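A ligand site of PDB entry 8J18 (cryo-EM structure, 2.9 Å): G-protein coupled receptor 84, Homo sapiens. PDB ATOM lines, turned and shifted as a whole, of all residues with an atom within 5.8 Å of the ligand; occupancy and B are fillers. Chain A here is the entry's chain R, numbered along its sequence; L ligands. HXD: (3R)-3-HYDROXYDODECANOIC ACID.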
ATOM      1  N   TYR A  79      31.615 -13.036  27.700  1.00  0.00           N
ATOM      2  CA  TYR A  79      31.951 -14.417  28.042  1.00  0.00           C
ATOM      3  C   TYR A  79      33.325 -14.514  28.688  1.00  0.00           C
ATOM      4  O   TYR A  79      33.488 -15.145  29.741  1.00  0.00           O
ATOM      5  CB  TYR A  79      31.890 -15.317  26.806  1.00  0.00           C
ATOM      6  CG  TYR A  79      32.402 -16.699  27.110  1.00  0.00           C
ATOM      7  CD1 TYR A  79      31.677 -17.569  27.906  1.00  0.00           C
ATOM      8  CD2 TYR A  79      33.621 -17.132  26.622  1.00  0.00           C
ATOM      9  CE1 TYR A  79      32.150 -18.833  28.201  1.00  0.00           C
ATOM     10  CE2 TYR A  79      34.098 -18.391  26.905  1.00  0.00           C
ATOM     11  CZ  TYR A  79      33.361 -19.239  27.699  1.00  0.00           C
ATOM     12  OH  TYR A  79      33.822 -20.491  27.996  1.00  0.00           O
ATOM     13  N   LEU A 110      25.871 -17.065  30.152  1.00  0.00           N
ATOM     14  CA  LEU A 110      26.723 -17.857  29.275  1.00  0.00           C
ATOM     15  C   LEU A 110      26.001 -18.185  27.969  1.00  0.00           C
ATOM     16  O   LEU A 110      26.514 -17.937  26.870  1.00  0.00           O
ATOM     17  CB  LEU A 110      27.135 -19.130  30.012  1.00  0.00           C
ATOM     18  CG  LEU A 110      27.712 -20.314  29.243  1.00  0.00           C
ATOM     19  CD1 LEU A 110      29.060 -19.946  28.644  1.00  0.00           C
ATOM     20  CD2 LEU A 110      27.852 -21.483  30.193  1.00  0.00           C
ATOM     21  N   PHE A 111      24.795 -18.742  28.081  1.00  0.00           N
ATOM     22  CA  PHE A 111      24.095 -19.138  26.870  1.00  0.00           C
ATOM     23  C   PHE A 111      23.630 -17.931  26.079  1.00  0.00           C
ATOM     24  O   PHE A 111      23.601 -17.965  24.845  1.00  0.00           O
ATOM     25  CB  PHE A 111      22.950 -20.069  27.227  1.00  0.00           C
ATOM     26  CG  PHE A 111      23.382 -21.491  27.412  1.00  0.00           C
ATOM     27  CD1 PHE A 111      24.215 -21.828  28.462  1.00  0.00           C
ATOM     28  CD2 PHE A 111      22.985 -22.481  26.538  1.00  0.00           C
ATOM     29  CE1 PHE A 111      24.638 -23.121  28.641  1.00  0.00           C
ATOM     30  CE2 PHE A 111      23.398 -23.783  26.719  1.00  0.00           C
ATOM     31  CZ  PHE A 111      24.230 -24.098  27.770  1.00  0.00           C
ATOM     32  N   ASN A 114      26.677 -16.826  24.090  1.00  0.00           N
ATOM     33  CA  ASN A 114      27.036 -17.751  23.002  1.00  0.00           C
ATOM     34  C   ASN A 114      26.016 -17.590  21.886  1.00  0.00           C
ATOM     35  O   ASN A 114      26.392 -17.645  20.736  1.00  0.00           O
ATOM     36  CB  ASN A 114      27.087 -19.220  23.470  1.00  0.00           C
ATOM     37  CG  ASN A 114      28.408 -19.573  24.126  1.00  0.00           C
ATOM     38  OD1 ASN A 114      29.066 -20.527  23.731  1.00  0.00           O
ATOM     39  ND2 ASN A 114      28.798 -18.817  25.138  1.00  0.00           N
ATOM     40  N   SER A 115      24.734 -17.401  22.215  1.00  0.00           N
ATOM     41  CA  SER A 115      23.718 -17.136  21.212  1.00  0.00           C
ATOM     42  C   SER A 115      23.952 -15.813  20.486  1.00  0.00           C
ATOM     43  O   SER A 115      23.776 -15.749  19.266  1.00  0.00           O
ATOM     44  CB  SER A 115      22.340 -17.135  21.850  1.00  0.00           C
ATOM     45  OG  SER A 115      22.363 -16.495  23.113  1.00  0.00           O
ATOM     46  N   ILE A 118      26.775 -16.363  18.012  1.00  0.00           N
ATOM     47  CA  ILE A 118      26.356 -17.117  16.830  1.00  0.00           C
ATOM     48  C   ILE A 118      25.539 -16.225  15.897  1.00  0.00           C
ATOM     49  O   ILE A 118      25.741 -16.207  14.674  1.00  0.00           O
ATOM     50  CB  ILE A 118      25.564 -18.364  17.243  1.00  0.00           C
ATOM     51  CG1 ILE A 118      26.498 -19.390  17.886  1.00  0.00           C
ATOM     52  CG2 ILE A 118      24.872 -18.980  16.032  1.00  0.00           C
ATOM     53  CD1 ILE A 118      25.776 -20.444  18.687  1.00  0.00           C
ATOM     54  N   PHE A 162      16.864 -18.071  26.000  1.00  0.00           N
ATOM     55  CA  PHE A 162      17.514 -18.715  27.136  1.00  0.00           C
ATOM     56  C   PHE A 162      17.098 -18.185  28.490  1.00  0.00           C
ATOM     57  O   PHE A 162      17.589 -18.678  29.509  1.00  0.00           O
ATOM     58  CB  PHE A 162      19.038 -18.595  26.976  1.00  0.00           C
ATOM     59  CG  PHE A 162      19.587 -19.458  25.893  1.00  0.00           C
ATOM     60  CD1 PHE A 162      19.575 -20.837  26.017  1.00  0.00           C
ATOM     61  CD2 PHE A 162      20.091 -18.907  24.733  1.00  0.00           C
ATOM     62  CE1 PHE A 162      20.067 -21.640  25.015  1.00  0.00           C
ATOM     63  CE2 PHE A 162      20.595 -19.713  23.725  1.00  0.00           C
ATOM     64  CZ  PHE A 162      20.576 -21.080  23.875  1.00  0.00           C
ATOM     65  N   VAL A 175      29.858 -31.417  32.777  1.00  0.00           N
ATOM     66  CA  VAL A 175      30.578 -30.255  32.268  1.00  0.00           C
ATOM     67  C   VAL A 175      31.308 -29.493  33.367  1.00  0.00           C
ATOM     68  O   VAL A 175      32.092 -28.596  33.054  1.00  0.00           O
ATOM     69  CB  VAL A 175      29.647 -29.314  31.483  1.00  0.00           C
ATOM     70  CG1 VAL A 175      30.460 -28.289  30.699  1.00  0.00           C
ATOM     71  CG2 VAL A 175      28.739 -30.111  30.563  1.00  0.00           C
ATOM     72  N   THR A 177      30.526 -27.160  35.077  1.00  0.00           N
ATOM     73  CA  THR A 177      30.203 -25.747  35.077  1.00  0.00           C
ATOM     74  C   THR A 177      28.692 -25.596  35.060  1.00  0.00           C
ATOM     75  O   THR A 177      27.967 -26.512  34.670  1.00  0.00           O
ATOM     76  CB  THR A 177      30.833 -25.005  33.890  1.00  0.00           C
ATOM     77  OG1 THR A 177      30.893 -23.602  34.167  1.00  0.00           O
ATOM     78  CG2 THR A 177      30.028 -25.234  32.628  1.00  0.00           C
ATOM     79  N   SER A 179      25.175 -24.748  33.925  1.00  0.00           N
ATOM     80  CA  SER A 179      24.465 -24.600  32.656  1.00  0.00           C
ATOM     81  C   SER A 179      23.134 -25.330  32.787  1.00  0.00           C
ATOM     82  O   SER A 179      22.770 -25.812  33.866  1.00  0.00           O
ATOM     83  CB  SER A 179      25.290 -25.148  31.489  1.00  0.00           C
ATOM     84  OG  SER A 179      25.629 -26.502  31.694  1.00  0.00           O
ATOM     85  N   ARG A 182      20.502 -31.247  31.434  1.00  0.00           N
ATOM     86  CA  ARG A 182      20.202 -31.893  30.160  1.00  0.00           C
ATOM     87  C   ARG A 182      18.911 -32.688  30.196  1.00  0.00           C
ATOM     88  O   ARG A 182      18.129 -32.650  29.241  1.00  0.00           O
ATOM     89  CB  ARG A 182      21.366 -32.800  29.758  1.00  0.00           C
ATOM     90  CG  ARG A 182      22.715 -32.105  29.648  1.00  0.00           C
ATOM     91  CD  ARG A 182      22.759 -31.115  28.482  1.00  0.00           C
ATOM     92  NE  ARG A 182      23.513 -29.912  28.829  1.00  0.00           N
ATOM     93  CZ  ARG A 182      24.834 -29.814  28.778  1.00  0.00           C
ATOM     94  NH1 ARG A 182      25.585 -30.836  28.408  1.00  0.00           N
ATOM     95  NH2 ARG A 182      25.410 -28.666  29.110  1.00  0.00           N
ATOM     96  N   THR A 189      15.249 -27.179  24.936  1.00  0.00           N
ATOM     97  CA  THR A 189      16.661 -26.871  24.748  1.00  0.00           C
ATOM     98  C   THR A 189      17.209 -27.568  23.498  1.00  0.00           C
ATOM     99  O   THR A 189      18.014 -26.980  22.763  1.00  0.00           O
ATOM    100  CB  THR A 189      17.473 -27.279  25.983  1.00  0.00           C
ATOM    101  OG1 THR A 189      18.757 -26.627  25.942  1.00  0.00           O
ATOM    102  CG2 THR A 189      17.690 -28.779  26.025  1.00  0.00           C
ATOM    103  N   LEU A 192      15.972 -25.643  20.500  1.00  0.00           N
ATOM    104  CA  LEU A 192      16.762 -24.427  20.386  1.00  0.00           C
ATOM    105  C   LEU A 192      18.133 -24.718  19.787  1.00  0.00           C
ATOM    106  O   LEU A 192      18.622 -23.997  18.910  1.00  0.00           O
ATOM    107  CB  LEU A 192      16.911 -23.775  21.761  1.00  0.00           C
ATOM    108  CG  LEU A 192      16.754 -22.262  21.924  1.00  0.00           C
ATOM    109  CD1 LEU A 192      15.704 -21.670  20.989  1.00  0.00           C
ATOM    110  CD2 LEU A 192      16.413 -21.953  23.378  1.00  0.00           C
ATOM    111  N   MET A 193      18.770 -25.784  20.269  1.00  0.00           N
ATOM    112  CA  MET A 193      20.094 -26.158  19.797  1.00  0.00           C
ATOM    113  C   MET A 193      20.063 -26.541  18.322  1.00  0.00           C
ATOM    114  O   MET A 193      20.954 -26.165  17.562  1.00  0.00           O
ATOM    115  CB  MET A 193      20.614 -27.322  20.641  1.00  0.00           C
ATOM    116  CG  MET A 193      21.352 -26.887  21.891  1.00  0.00           C
ATOM    117  SD  MET A 193      21.893 -28.248  22.957  1.00  0.00           S
ATOM    118  CE  MET A 193      21.488 -29.690  21.979  1.00  0.00           C
ATOM    119  N   TYR A 196      19.672 -23.363  16.257  1.00  0.00           N
ATOM    120  CA  TYR A 196      20.930 -22.623  16.168  1.00  0.00           C
ATOM    121  C   TYR A 196      21.938 -23.332  15.266  1.00  0.00           C
ATOM    122  O   TYR A 196      22.617 -22.678  14.475  1.00  0.00           O
ATOM    123  CB  TYR A 196      21.516 -22.408  17.554  1.00  0.00           C
ATOM    124  CG  TYR A 196      21.181 -21.053  18.135  1.00  0.00           C
ATOM    125  CD1 TYR A 196      21.892 -19.932  17.755  1.00  0.00           C
ATOM    126  CD2 TYR A 196      20.145 -20.908  19.047  1.00  0.00           C
ATOM    127  CE1 TYR A 196      21.590 -18.689  18.283  1.00  0.00           C
ATOM    128  CE2 TYR A 196      19.836 -19.670  19.564  1.00  0.00           C
ATOM    129  CZ  TYR A 196      20.558 -18.570  19.186  1.00  0.00           C
ATOM    130  OH  TYR A 196      20.250 -17.333  19.703  1.00  0.00           O
ATOM    131  N   TYR A 342      31.403 -24.829  17.450  1.00  0.00           N
ATOM    132  CA  TYR A 342      30.062 -25.220  17.947  1.00  0.00           C
ATOM    133  C   TYR A 342      29.512 -26.547  17.534  1.00  0.00           C
ATOM    134  O   TYR A 342      28.845 -27.161  18.344  1.00  0.00           O
ATOM    135  CB  TYR A 342      29.023 -24.176  17.584  1.00  0.00           C
ATOM    136  CG  TYR A 342      29.145 -22.889  18.342  1.00  0.00           C
ATOM    137  CD1 TYR A 342      29.020 -22.855  19.735  1.00  0.00           C
ATOM    138  CD2 TYR A 342      29.353 -21.701  17.681  1.00  0.00           C
ATOM    139  CE1 TYR A 342      29.124 -21.671  20.433  1.00  0.00           C
ATOM    140  CE2 TYR A 342      29.473 -20.533  18.368  1.00  0.00           C
ATOM    141  CZ  TYR A 342      29.352 -20.507  19.743  1.00  0.00           C
ATOM    142  OH  TYR A 342      29.450 -19.319  20.426  1.00  0.00           O
ATOM    143  N   PHE A 345      29.723 -29.454  20.243  1.00  0.00           N
ATOM    144  CA  PHE A 345      28.861 -29.323  21.407  1.00  0.00           C
ATOM    145  C   PHE A 345      27.401 -29.511  21.024  1.00  0.00           C
ATOM    146  O   PHE A 345      26.680 -30.326  21.625  1.00  0.00           O
ATOM    147  CB  PHE A 345      29.081 -27.952  22.042  1.00  0.00           C
ATOM    148  CG  PHE A 345      28.307 -27.721  23.312  1.00  0.00           C
ATOM    149  CD1 PHE A 345      28.685 -28.336  24.490  1.00  0.00           C
ATOM    150  CD2 PHE A 345      27.190 -26.901  23.324  1.00  0.00           C
ATOM    151  CE1 PHE A 345      27.982 -28.133  25.657  1.00  0.00           C
ATOM    152  CE2 PHE A 345      26.477 -26.698  24.488  1.00  0.00           C
ATOM    153  CZ  PHE A 345      26.877 -27.307  25.659  1.00  0.00           C
ATOM    154  N   LEU A 346      26.953 -28.790  20.005  1.00  0.00           N
ATOM    155  CA  LEU A 346      25.544 -28.820  19.612  1.00  0.00           C
ATOM    156  C   LEU A 346      25.127 -30.235  19.233  1.00  0.00           C
ATOM    157  O   LEU A 346      24.110 -30.731  19.715  1.00  0.00           O
ATOM    158  CB  LEU A 346      25.309 -27.860  18.455  1.00  0.00           C
ATOM    159  CG  LEU A 346      25.501 -26.373  18.757  1.00  0.00           C
ATOM    160  CD1 LEU A 346      25.553 -25.590  17.471  1.00  0.00           C
ATOM    161  CD2 LEU A 346      24.388 -25.862  19.650  1.00  0.00           C
ATOM    162  N   ALA A 366      32.363 -28.933  25.365  1.00  0.00           N
ATOM    163  CA  ALA A 366      32.150 -27.618  25.966  1.00  0.00           C
ATOM    164  C   ALA A 366      33.383 -26.743  25.808  1.00  0.00           C
ATOM    165  O   ALA A 366      33.277 -25.545  25.515  1.00  0.00           O
ATOM    166  CB  ALA A 366      31.799 -27.777  27.449  1.00  0.00           C
ATOM    167  N   ASN A 367      34.568 -27.319  25.979  1.00  0.00           N
ATOM    168  CA  ASN A 367      35.807 -26.553  25.873  1.00  0.00           C
ATOM    169  C   ASN A 367      35.990 -26.002  24.469  1.00  0.00           C
ATOM    170  O   ASN A 367      36.447 -24.864  24.303  1.00  0.00           O
ATOM    171  CB  ASN A 367      36.994 -27.432  26.250  1.00  0.00           C
ATOM    172  CG  ASN A 367      37.039 -27.736  27.734  1.00  0.00           C
ATOM    173  OD1 ASN A 367      36.309 -27.142  28.521  1.00  0.00           O
ATOM    174  ND2 ASN A 367      37.877 -28.687  28.120  1.00  0.00           N
ATOM    175  N   THR A 369      33.785 -24.910  22.554  1.00  0.00           N
ATOM    176  CA  THR A 369      32.988 -23.685  22.442  1.00  0.00           C
ATOM    177  C   THR A 369      33.735 -22.480  23.014  1.00  0.00           C
ATOM    178  O   THR A 369      33.406 -21.353  22.642  1.00  0.00           O
ATOM    179  CB  THR A 369      31.551 -23.742  23.043  1.00  0.00           C
ATOM    180  OG1 THR A 369      31.591 -23.546  24.468  1.00  0.00           O
ATOM    181  CG2 THR A 369      30.777 -25.037  22.686  1.00  0.00           C
ATOM    182  N   TRP A 370      34.756 -22.695  23.859  1.00  0.00           N
ATOM    183  CA  TRP A 370      35.543 -21.555  24.337  1.00  0.00           C
ATOM    184  C   TRP A 370      36.422 -20.986  23.245  1.00  0.00           C
ATOM    185  O   TRP A 370      36.916 -19.859  23.379  1.00  0.00           O
ATOM    186  CB  TRP A 370      36.408 -21.961  25.529  1.00  0.00           C
ATOM    187  CG  TRP A 370      35.698 -22.708  26.627  1.00  0.00           C
ATOM    188  CD1 TRP A 370      34.362 -22.988  26.710  1.00  0.00           C
ATOM    189  CD2 TRP A 370      36.295 -23.294  27.788  1.00  0.00           C
ATOM    190  NE1 TRP A 370      34.093 -23.697  27.853  1.00  0.00           N
ATOM    191  CE2 TRP A 370      35.271 -23.893  28.531  1.00  0.00           C
ATOM    192  CE3 TRP A 370      37.604 -23.352  28.272  1.00  0.00           C
ATOM    193  CZ2 TRP A 370      35.501 -24.559  29.734  1.00  0.00           C
ATOM    194  CZ3 TRP A 370      37.835 -24.008  29.470  1.00  0.00           C
ATOM    195  CH2 TRP A 370      36.797 -24.598  30.182  1.00  0.00           C
HETATM  196  C11 HXD L   1      22.983 -22.476  20.752  1.00  0.00           C
HETATM  197  C10 HXD L   1      23.692 -21.370  21.541  1.00  0.00           C
HETATM  198  C12 HXD L   1      22.073 -23.281  21.680  1.00  0.00           C
HETATM  199  C9  HXD L   1      24.657 -22.008  22.539  1.00  0.00           C
HETATM  200  C8  HXD L   1      25.246 -23.271  21.912  1.00  0.00           C
HETATM  201  C7  HXD L   1      26.409 -23.748  22.771  1.00  0.00           C
HETATM  202  C6  HXD L   1      26.080 -23.488  24.239  1.00  0.00           C
HETATM  203  C5  HXD L   1      27.324 -22.961  24.949  1.00  0.00           C
HETATM  204  C4  HXD L   1      27.864 -24.004  25.915  1.00  0.00           C
HETATM  205  C3  HXD L   1      29.265 -23.589  26.336  1.00  0.00           C
HETATM  206  O8  HXD L   1      29.526 -22.307  25.840  1.00  0.00           O
HETATM  207  C2  HXD L   1      29.366 -23.561  27.856  1.00  0.00           C
HETATM  208  C1  HXD L   1      29.153 -24.958  28.441  1.00  0.00           C
HETATM  209  O1  HXD L   1      30.093 -25.533  29.038  1.00  0.00           O
HETATM  210  O   HXD L   1      28.039 -25.532  28.325  1.00  0.00           O
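Merely in contact with the ligand: Leu 110, Phe 111, Ile 118, Phe 162, Val 175, Thr 177, Met 193, Tyr 196, Phe 345, Leu 346 and Ala 366.
Hydrophobic or aromatic side chains that line the ligand: Leu 110, Phe 111, Ile 118, Phe 162, Val 175, Met 193, Tyr 196, Phe 345, Leu 346 and Ala 366.
Within 4 Å of the ligand: Leu 110, Phe 111, Asn 114, Ile 118, Phe 162, Val 175, Thr 177, Met 193, Tyr 196, Phe 345, Leu 346, Ala 366 and Thr 369.
The side-chain hydroxyl of Thr 369 sits at hydrogen-bond distance from the backbone carbonyl oxygen of Ala 366 (2.8 Å).
The side-chain amide nitrogen (ND2) of Asn 114 lies within hydrogen-bond range of the backbone carbonyl oxygen (O) of Leu 110 (3.0 Å).
The backbone carbonyl oxygen (O) of Ala 366 lies close to the indole nitrogen (NE1) of Trp 370, at 3.1 Å.
The backbone carbonyl oxygen (O) of Phe 111 sits at hydrogen-bond distance from the side-chain hydroxyl (OG) of Ser 115 (2.6 Å).
The side-chain amide oxygen (OD1) of Asn 114 sits at hydrogen-bond distance from an oxygen (O8) of the ligand (2.8 Å).
OG1 of Thr 369 lies within hydrogen-bond range of O8 of the ligand, 2.8 Å away.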
